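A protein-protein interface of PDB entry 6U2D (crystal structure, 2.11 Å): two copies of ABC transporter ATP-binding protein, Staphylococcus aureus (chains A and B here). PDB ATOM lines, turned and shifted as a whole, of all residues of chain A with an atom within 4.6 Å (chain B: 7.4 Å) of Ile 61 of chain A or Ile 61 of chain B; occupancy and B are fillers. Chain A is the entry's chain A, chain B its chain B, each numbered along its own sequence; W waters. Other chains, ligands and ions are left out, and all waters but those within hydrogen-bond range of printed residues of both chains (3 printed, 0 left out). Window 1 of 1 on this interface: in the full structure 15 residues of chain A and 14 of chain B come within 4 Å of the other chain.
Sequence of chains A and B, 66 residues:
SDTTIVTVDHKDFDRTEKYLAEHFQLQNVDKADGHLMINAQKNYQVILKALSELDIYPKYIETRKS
Among the printed residues, merely in contact across the chains: Tyr 60 of chain A with Thr 63 of chain B (3.6 Å), Ile 61 of chain A with Tyr 44 of chain B (3.6 Å), Tyr 44 of chain A with Ile 61 of chain B (3.7 Å), Tyr 44 of chain A with Pro 58 of chain B (3.7 Å) and Ile 61 of chain A with Ile 61 of chain B (3.8 Å).
Ile 5 of chain A touches none of the printed residues of chain B. Printed residues of chain B within 4 Å of Tyr 44 of chain A: Pro 58, Lys 59, Tyr 60 and Ile 61. Printed residues of chain B within 4 Å of Tyr 60 of chain A: Tyr 44 and Thr 63. Of the printed residues of chain A, Tyr 44 of chain B touches Tyr 60 (3.4 Å) and Ile 61 (3.6 Å). Printed residues of chain A within 4 Å of Lys 59 of chain B: Tyr 44. Of the printed residues of chain A, Tyr 60 of chain B touches Tyr 44 (3.4 Å). Ile 61 of chain B touches just these residues of chain A: Tyr 44 and Ile 61. The nearest residue of chain B that does not touch Ile 61 of chain A is Leu 48 of chain B (5.1 Å). The nearest printed residue of chain A that does not touch Ile 61 of chain B is Glu 62 of chain A (5.4 Å). The nearest printed residue of chain B that does not touch Tyr 44 of chain A is Glu 62 of chain B (5.8 Å).
Of the 7 printed residues of chain A, 3 touch a printed residue of chain B. Hydrophobic or aromatic side chains of chain A that line the printed part of chain B: Tyr 44, Tyr 60 and Ile 61. Along chain A the printed residues that touch a printed residue of chain B span positions 44 to 61. Among the printed residues, no Asp or Glu carboxylate lies within 4 Å of a Lys or Arg side-chain nitrogen of the other chain.
Tyr 44 of chain A touches Tyr 60 of chain B, and with the chains exchanged Tyr 60 of chain A touches Tyr 44 of chain B. Tyr 44 of chain A touches Ile 61 of chain B, and with the chains exchanged Ile 61 of chain A touches Tyr 44 of chain B. Ile 61 of chain B touches its own counterpart, Ile 61 of chain A. 7 positions are printed for both chains.
Water W2 bridges the side-chain hydroxyl of Tyr 44 of chain A (2.6 Å) and the backbone carbonyl oxygen of Ile 61 of chain B (2.6 Å). Water W3 lies within hydrogen-bond range of OH of Tyr 44 of chain B (2.6 Å), O of Ile 61 of chain A (2.7 Å) and O of Ile 61 of chain B (3.1 Å). Water W1 bridges N of Thr 63 of chain B (3.0 Å) and OH of Tyr 60 of chain A (3.4 Å).
The side-chain hydroxyl of Thr 63 of chain B sits at hydrogen-bond distance from the side-chain hydroxyl of Thr 4 of chain B (3.0 Å). The backbone carbonyl oxygen (O) of Thr 7 of chain B lies within hydrogen-bond range of the backbone NH (N) of Lys 59 of chain B. O of Tyr 60 of chain B lies within hydrogen-bond range of N of Thr 7 of chain B. OG1 of Thr 63 of chain B sits at hydrogen-bond distance from OH of Tyr 44 of chain B.
The backbone carbonyl oxygen (O) of Lys 59 of chain B is in hydrogen-bond range of the backbone NH (N) of Tyr 44 of chain A, at 2.7 Å. OH of Tyr 44 of chain A lies within hydrogen-bond range of OH of Tyr 60 of chain B, at 3.4 Å. OH of Tyr 44 of chain B is in hydrogen-bond range of OH of Tyr 60 of chain A (3.4 Å).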
ATOM      1  N   THR A   4      16.972 -22.260 -23.555  1.00  0.00           N
ATOM      2  CA  THR A   4      16.039 -22.590 -24.630  1.00  0.00           C
ATOM      3  C   THR A   4      16.676 -22.298 -25.985  1.00  0.00           C
ATOM      4  O   THR A   4      17.231 -21.213 -26.190  1.00  0.00           O
ATOM      5  CB  THR A   4      14.730 -21.802 -24.504  1.00  0.00           C
ATOM      6  OG1 THR A   4      13.970 -22.262 -23.374  1.00  0.00           O
ATOM      7  CG2 THR A   4      13.901 -21.970 -25.757  1.00  0.00           C
ATOM      8  N   ILE A   5      16.616 -23.263 -26.898  1.00  0.00           N
ATOM      9  CA  ILE A   5      17.205 -23.151 -28.229  1.00  0.00           C
ATOM     10  C   ILE A   5      16.090 -23.084 -29.269  1.00  0.00           C
ATOM     11  O   ILE A   5      15.270 -24.008 -29.381  1.00  0.00           O
ATOM     12  CB  ILE A   5      18.130 -24.336 -28.549  1.00  0.00           C
ATOM     13  CG1 ILE A   5      19.117 -24.628 -27.415  1.00  0.00           C
ATOM     14  CG2 ILE A   5      18.845 -24.095 -29.886  1.00  0.00           C
ATOM     15  CD1 ILE A   5      19.899 -23.418 -26.932  1.00  0.00           C
ATOM     16  N   VAL A   6      16.107 -22.034 -30.085  1.00  0.00           N
ATOM     17  CA  VAL A   6      15.176 -21.858 -31.192  1.00  0.00           C
ATOM     18  C   VAL A   6      15.931 -22.117 -32.489  1.00  0.00           C
ATOM     19  O   VAL A   6      16.990 -21.521 -32.725  1.00  0.00           O
ATOM     20  CB  VAL A   6      14.573 -20.443 -31.179  1.00  0.00           C
ATOM     21  CG1 VAL A   6      13.595 -20.256 -32.351  1.00  0.00           C
ATOM     22  CG2 VAL A   6      13.885 -20.186 -29.846  1.00  0.00           C
ATOM     23  N   TYR A  44       6.019 -21.539 -24.175  1.00  0.00           N
ATOM     24  CA  TYR A  44       6.437 -21.126 -25.512  1.00  0.00           C
ATOM     25  C   TYR A  44       5.440 -20.212 -26.230  1.00  0.00           C
ATOM     26  O   TYR A  44       5.712 -19.820 -27.367  1.00  0.00           O
ATOM     27  CB  TYR A  44       6.691 -22.356 -26.399  1.00  0.00           C
ATOM     28  CG  TYR A  44       7.881 -23.230 -26.029  1.00  0.00           C
ATOM     29  CD1 TYR A  44       8.856 -22.792 -25.140  1.00  0.00           C
ATOM     30  CD2 TYR A  44       7.999 -24.524 -26.545  1.00  0.00           C
ATOM     31  CE1 TYR A  44       9.944 -23.601 -24.805  1.00  0.00           C
ATOM     32  CE2 TYR A  44       9.073 -25.346 -26.201  1.00  0.00           C
ATOM     33  CZ  TYR A  44      10.047 -24.876 -25.337  1.00  0.00           C
ATOM     34  OH  TYR A  44      11.129 -25.682 -24.997  1.00  0.00           O
ATOM     35  N   TYR A  60      12.542 -26.201 -34.991  1.00  0.00           N
ATOM     36  CA  TYR A  60      12.674 -26.877 -33.712  1.00  0.00           C
ATOM     37  C   TYR A  60      12.719 -25.840 -32.607  1.00  0.00           C
ATOM     38  O   TYR A  60      13.047 -24.673 -32.831  1.00  0.00           O
ATOM     39  CB  TYR A  60      13.935 -27.735 -33.654  1.00  0.00           C
ATOM     40  CG  TYR A  60      13.756 -29.002 -32.868  1.00  0.00           C
ATOM     41  CD1 TYR A  60      13.092 -30.094 -33.417  1.00  0.00           C
ATOM     42  CD2 TYR A  60      14.225 -29.102 -31.566  1.00  0.00           C
ATOM     43  CE1 TYR A  60      12.926 -31.279 -32.694  1.00  0.00           C
ATOM     44  CE2 TYR A  60      14.057 -30.280 -30.828  1.00  0.00           C
ATOM     45  CZ  TYR A  60      13.411 -31.358 -31.396  1.00  0.00           C
ATOM     46  OH  TYR A  60      13.252 -32.514 -30.653  1.00  0.00           O
ATOM     47  N   ILE A  61      12.359 -26.278 -31.410  1.00  0.00           N
ATOM     48  CA  ILE A  61      12.522 -25.463 -30.215  1.00  0.00           C
ATOM     49  C   ILE A  61      12.638 -26.435 -29.061  1.00  0.00           C
ATOM     50  O   ILE A  61      11.901 -27.422 -29.010  1.00  0.00           O
ATOM     51  CB  ILE A  61      11.359 -24.461 -30.017  1.00  0.00           C
ATOM     52  CG1 ILE A  61      11.484 -23.715 -28.695  1.00  0.00           C
ATOM     53  CG2 ILE A  61       9.980 -25.163 -30.074  1.00  0.00           C
ATOM     54  CD1 ILE A  61      10.616 -22.456 -28.667  1.00  0.00           C
ATOM     55  N   GLU A  62      13.601 -26.215 -28.175  1.00  0.00           N
ATOM     56  CA  GLU A  62      13.802 -27.152 -27.084  1.00  0.00           C
ATOM     57  C   GLU A  62      14.504 -26.453 -25.938  1.00  0.00           C
ATOM     58  O   GLU A  62      15.125 -25.402 -26.116  1.00  0.00           O
ATOM     59  CB  GLU A  62      14.576 -28.383 -27.546  1.00  0.00           C
ATOM     60  CG  GLU A  62      16.033 -28.169 -27.802  1.00  0.00           C
ATOM     61  CD  GLU A  62      16.730 -29.483 -28.081  1.00  0.00           C
ATOM     62  OE1 GLU A  62      17.292 -29.646 -29.182  1.00  0.00           O
ATOM     63  OE2 GLU A  62      16.667 -30.375 -27.207  1.00  0.00           O
ATOM     64  N   THR B   4       6.474 -37.176 -29.856  1.00  0.00           N
ATOM     65  CA  THR B   4       6.335 -35.737 -29.726  1.00  0.00           C
ATOM     66  C   THR B   4       5.097 -35.411 -28.901  1.00  0.00           C
ATOM     67  O   THR B   4       3.997 -35.886 -29.203  1.00  0.00           O
ATOM     68  CB  THR B   4       6.251 -35.094 -31.117  1.00  0.00           C
ATOM     69  OG1 THR B   4       7.534 -35.167 -31.759  1.00  0.00           O
ATOM     70  CG2 THR B   4       5.795 -33.635 -31.035  1.00  0.00           C
ATOM     71  N   ILE B   5       5.286 -34.610 -27.857  1.00  0.00           N
ATOM     72  CA  ILE B   5       4.220 -34.229 -26.938  1.00  0.00           C
ATOM     73  C   ILE B   5       3.929 -32.747 -27.114  1.00  0.00           C
ATOM     74  O   ILE B   5       4.823 -31.904 -26.949  1.00  0.00           O
ATOM     75  CB  ILE B   5       4.586 -34.554 -25.484  1.00  0.00           C
ATOM     76  CG1 ILE B   5       5.002 -36.023 -25.371  1.00  0.00           C
ATOM     77  CG2 ILE B   5       3.442 -34.206 -24.563  1.00  0.00           C
ATOM     78  CD1 ILE B   5       5.846 -36.324 -24.160  1.00  0.00           C
ATOM     79  N   VAL B   6       2.670 -32.435 -27.416  1.00  0.00           N
ATOM     80  CA  VAL B   6       2.176 -31.071 -27.570  1.00  0.00           C
ATOM     81  C   VAL B   6       1.335 -30.734 -26.345  1.00  0.00           C
ATOM     82  O   VAL B   6       0.431 -31.502 -25.974  1.00  0.00           O
ATOM     83  CB  VAL B   6       1.353 -30.922 -28.864  1.00  0.00           C
ATOM     84  CG1 VAL B   6       0.820 -29.493 -29.033  1.00  0.00           C
ATOM     85  CG2 VAL B   6       2.186 -31.325 -30.067  1.00  0.00           C
ATOM     86  N   THR B   7       1.631 -29.592 -25.715  1.00  0.00           N
ATOM     87  CA  THR B   7       0.916 -29.114 -24.534  1.00  0.00           C
ATOM     88  C   THR B   7       0.239 -27.780 -24.846  1.00  0.00           C
ATOM     89  O   THR B   7       0.883 -26.854 -25.346  1.00  0.00           O
ATOM     90  CB  THR B   7       1.879 -28.997 -23.348  1.00  0.00           C
ATOM     91  OG1 THR B   7       2.508 -30.267 -23.139  1.00  0.00           O
ATOM     92  CG2 THR B   7       1.182 -28.540 -22.058  1.00  0.00           C
ATOM     93  N   ILE B  38       1.848 -37.539 -30.091  1.00  0.00           N
ATOM     94  CA  ILE B  38       1.720 -37.974 -31.474  1.00  0.00           C
ATOM     95  C   ILE B  38       3.041 -38.608 -31.880  1.00  0.00           C
ATOM     96  O   ILE B  38       4.007 -38.621 -31.113  1.00  0.00           O
ATOM     97  CB  ILE B  38       1.352 -36.821 -32.433  1.00  0.00           C
ATOM     98  CG1 ILE B  38       2.448 -35.741 -32.453  1.00  0.00           C
ATOM     99  CG2 ILE B  38       0.009 -36.211 -32.063  1.00  0.00           C
ATOM    100  CD1 ILE B  38       2.273 -34.731 -33.574  1.00  0.00           C
ATOM    101  N   GLN B  41       7.738 -35.775 -34.612  1.00  0.00           N
ATOM    102  CA  GLN B  41       7.925 -34.868 -35.732  1.00  0.00           C
ATOM    103  C   GLN B  41       9.380 -34.399 -35.651  1.00  0.00           C
ATOM    104  O   GLN B  41       9.773 -33.767 -34.667  1.00  0.00           O
ATOM    105  CB  GLN B  41       6.969 -33.677 -35.630  1.00  0.00           C
ATOM    106  CG  GLN B  41       5.450 -33.981 -35.532  1.00  0.00           C
ATOM    107  CD  GLN B  41       4.852 -34.494 -36.825  1.00  0.00           C
ATOM    108  OE1 GLN B  41       5.027 -33.894 -37.884  1.00  0.00           O
ATOM    109  NE2 GLN B  41       4.115 -35.599 -36.739  1.00  0.00           N
ATOM    110  N   ASN B  43      10.775 -32.201 -37.625  1.00  0.00           N
ATOM    111  CA  ASN B  43      10.709 -30.781 -37.933  1.00  0.00           C
ATOM    112  C   ASN B  43       9.326 -30.290 -37.522  1.00  0.00           C
ATOM    113  O   ASN B  43       8.312 -30.825 -37.990  1.00  0.00           O
ATOM    114  CB  ASN B  43      10.968 -30.560 -39.427  1.00  0.00           C
ATOM    115  CG  ASN B  43      10.938 -29.096 -39.843  1.00  0.00           C
ATOM    116  OD1 ASN B  43      10.102 -28.307 -39.393  1.00  0.00           O
ATOM    117  ND2 ASN B  43      11.833 -28.739 -40.756  1.00  0.00           N
ATOM    118  N   TYR B  44       9.281 -29.272 -36.657  1.00  0.00           N
ATOM    119  CA  TYR B  44       8.025 -28.819 -36.056  1.00  0.00           C
ATOM    120  C   TYR B  44       7.249 -27.826 -36.908  1.00  0.00           C
ATOM    121  O   TYR B  44       6.174 -27.398 -36.493  1.00  0.00           O
ATOM    122  CB  TYR B  44       8.278 -28.141 -34.705  1.00  0.00           C
ATOM    123  CG  TYR B  44       8.757 -29.009 -33.570  1.00  0.00           C
ATOM    124  CD1 TYR B  44       8.713 -30.387 -33.636  1.00  0.00           C
ATOM    125  CD2 TYR B  44       9.277 -28.422 -32.419  1.00  0.00           C
ATOM    126  CE1 TYR B  44       9.160 -31.164 -32.570  1.00  0.00           C
ATOM    127  CE2 TYR B  44       9.734 -29.180 -31.362  1.00  0.00           C
ATOM    128  CZ  TYR B  44       9.670 -30.546 -31.435  1.00  0.00           C
ATOM    129  OH  TYR B  44      10.109 -31.280 -30.357  1.00  0.00           O
ATOM    130  N   ILE B  47       3.344 -28.712 -37.953  1.00  0.00           N
ATOM    131  CA  ILE B  47       2.383 -28.742 -36.851  1.00  0.00           C
ATOM    132  C   ILE B  47       2.211 -27.350 -36.253  1.00  0.00           C
ATOM    133  O   ILE B  47       1.086 -26.927 -35.957  1.00  0.00           O
ATOM    134  CB  ILE B  47       2.757 -29.792 -35.789  1.00  0.00           C
ATOM    135  CG1 ILE B  47       1.596 -29.943 -34.812  1.00  0.00           C
ATOM    136  CG2 ILE B  47       3.942 -29.386 -34.995  1.00  0.00           C
ATOM    137  CD1 ILE B  47       1.685 -31.175 -33.935  1.00  0.00           C
ATOM    138  N   LEU B  48       3.305 -26.601 -36.091  1.00  0.00           N
ATOM    139  CA  LEU B  48       3.158 -25.292 -35.470  1.00  0.00           C
ATOM    140  C   LEU B  48       2.383 -24.359 -36.377  1.00  0.00           C
ATOM    141  O   LEU B  48       1.544 -23.586 -35.905  1.00  0.00           O
ATOM    142  CB  LEU B  48       4.522 -24.689 -35.128  1.00  0.00           C
ATOM    143  CG  LEU B  48       5.312 -25.424 -34.052  1.00  0.00           C
ATOM    144  CD1 LEU B  48       6.744 -24.869 -33.948  1.00  0.00           C
ATOM    145  CD2 LEU B  48       4.568 -25.353 -32.720  1.00  0.00           C
ATOM    146  N   LEU B  51      -1.488 -25.424 -36.283  1.00  0.00           N
ATOM    147  CA  LEU B  51      -2.137 -25.003 -35.044  1.00  0.00           C
ATOM    148  C   LEU B  51      -2.297 -23.484 -34.990  1.00  0.00           C
ATOM    149  O   LEU B  51      -3.299 -22.973 -34.465  1.00  0.00           O
ATOM    150  CB  LEU B  51      -1.329 -25.503 -33.849  1.00  0.00           C
ATOM    151  CG  LEU B  51      -1.334 -27.025 -33.668  1.00  0.00           C
ATOM    152  CD1 LEU B  51      -0.492 -27.449 -32.466  1.00  0.00           C
ATOM    153  CD2 LEU B  51      -2.775 -27.564 -33.552  1.00  0.00           C
ATOM    154  N   PRO B  58       1.113 -23.615 -28.801  1.00  0.00           N
ATOM    155  CA  PRO B  58       1.405 -24.517 -27.682  1.00  0.00           C
ATOM    156  C   PRO B  58       2.058 -23.790 -26.513  1.00  0.00           C
ATOM    157  O   PRO B  58       2.880 -22.887 -26.692  1.00  0.00           O
ATOM    158  CB  PRO B  58       2.366 -25.546 -28.295  1.00  0.00           C
ATOM    159  CG  PRO B  58       2.128 -25.489 -29.755  1.00  0.00           C
ATOM    160  CD  PRO B  58       1.709 -24.077 -30.067  1.00  0.00           C
ATOM    161  N   LYS B  59       1.658 -24.184 -25.305  1.00  0.00           N
ATOM    162  CA  LYS B  59       2.439 -23.839 -24.130  1.00  0.00           C
ATOM    163  C   LYS B  59       3.812 -24.492 -24.195  1.00  0.00           C
ATOM    164  O   LYS B  59       4.799 -23.927 -23.704  1.00  0.00           O
ATOM    165  CB  LYS B  59       1.711 -24.266 -22.861  1.00  0.00           C
ATOM    166  CG  LYS B  59       0.417 -23.534 -22.625  1.00  0.00           C
ATOM    167  CD  LYS B  59      -0.289 -24.139 -21.431  1.00  0.00           C
ATOM    168  CE  LYS B  59       0.604 -23.977 -20.217  1.00  0.00           C
ATOM    169  NZ  LYS B  59       0.092 -24.698 -19.034  1.00  0.00           N
ATOM    170  N   TYR B  60       3.885 -25.684 -24.781  1.00  0.00           N
ATOM    171  CA  TYR B  60       5.125 -26.438 -24.835  1.00  0.00           C
ATOM    172  C   TYR B  60       5.044 -27.463 -25.954  1.00  0.00           C
ATOM    173  O   TYR B  60       3.951 -27.906 -26.325  1.00  0.00           O
ATOM    174  CB  TYR B  60       5.390 -27.120 -23.493  1.00  0.00           C
ATOM    175  CG  TYR B  60       6.851 -27.219 -23.145  1.00  0.00           C
ATOM    176  CD1 TYR B  60       7.564 -26.085 -22.714  1.00  0.00           C
ATOM    177  CD2 TYR B  60       7.522 -28.434 -23.221  1.00  0.00           C
ATOM    178  CE1 TYR B  60       8.921 -26.160 -22.383  1.00  0.00           C
ATOM    179  CE2 TYR B  60       8.879 -28.521 -22.892  1.00  0.00           C
ATOM    180  CZ  TYR B  60       9.563 -27.376 -22.463  1.00  0.00           C
ATOM    181  OH  TYR B  60      10.887 -27.450 -22.137  1.00  0.00           O
ATOM    182  N   ILE B  61       6.213 -27.857 -26.461  1.00  0.00           N
ATOM    183  CA  ILE B  61       6.318 -28.975 -27.398  1.00  0.00           C
ATOM    184  C   ILE B  61       7.692 -29.604 -27.214  1.00  0.00           C
ATOM    185  O   ILE B  61       8.706 -28.897 -27.117  1.00  0.00           O
ATOM    186  CB  ILE B  61       6.087 -28.552 -28.866  1.00  0.00           C
ATOM    187  CG1 ILE B  61       6.309 -29.733 -29.811  1.00  0.00           C
ATOM    188  CG2 ILE B  61       7.010 -27.422 -29.277  1.00  0.00           C
ATOM    189  CD1 ILE B  61       5.686 -29.518 -31.171  1.00  0.00           C
ATOM    190  N   GLU B  62       7.723 -30.933 -27.117  1.00  0.00           N
ATOM    191  CA  GLU B  62       8.976 -31.619 -26.836  1.00  0.00           C
ATOM    192  C   GLU B  62       8.894 -33.052 -27.336  1.00  0.00           C
ATOM    193  O   GLU B  62       7.805 -33.608 -27.532  1.00  0.00           O
ATOM    194  CB  GLU B  62       9.309 -31.583 -25.346  1.00  0.00           C
ATOM    195  CG  GLU B  62       8.534 -32.544 -24.514  1.00  0.00           C
ATOM    196  CD  GLU B  62       8.976 -32.523 -23.076  1.00  0.00           C
ATOM    197  OE1 GLU B  62      10.192 -32.684 -22.817  1.00  0.00           O
ATOM    198  OE2 GLU B  62       8.096 -32.377 -22.202  1.00  0.00           O
ATOM    199  N   THR B  63      10.068 -33.636 -27.550  1.00  0.00           N
ATOM    200  CA  THR B  63      10.192 -34.998 -28.047  1.00  0.00           C
ATOM    201  C   THR B  63      10.979 -35.836 -27.051  1.00  0.00           C
ATOM    202  O   THR B  63      12.137 -35.519 -26.762  1.00  0.00           O
ATOM    203  CB  THR B  63      10.881 -34.993 -29.414  1.00  0.00           C
ATOM    204  OG1 THR B  63      10.060 -34.302 -30.366  1.00  0.00           O
ATOM    205  CG2 THR B  63      11.174 -36.400 -29.892  1.00  0.00           C
HETATM  206  O   HOH W   1      12.647 -32.053 -27.322  1.00  0.00           O
HETATM  207  O   HOH W   2      10.695 -28.157 -25.620  1.00  0.00           O
HETATM  208  O   HOH W   3      11.296 -30.006 -28.434  1.00  0.00           O
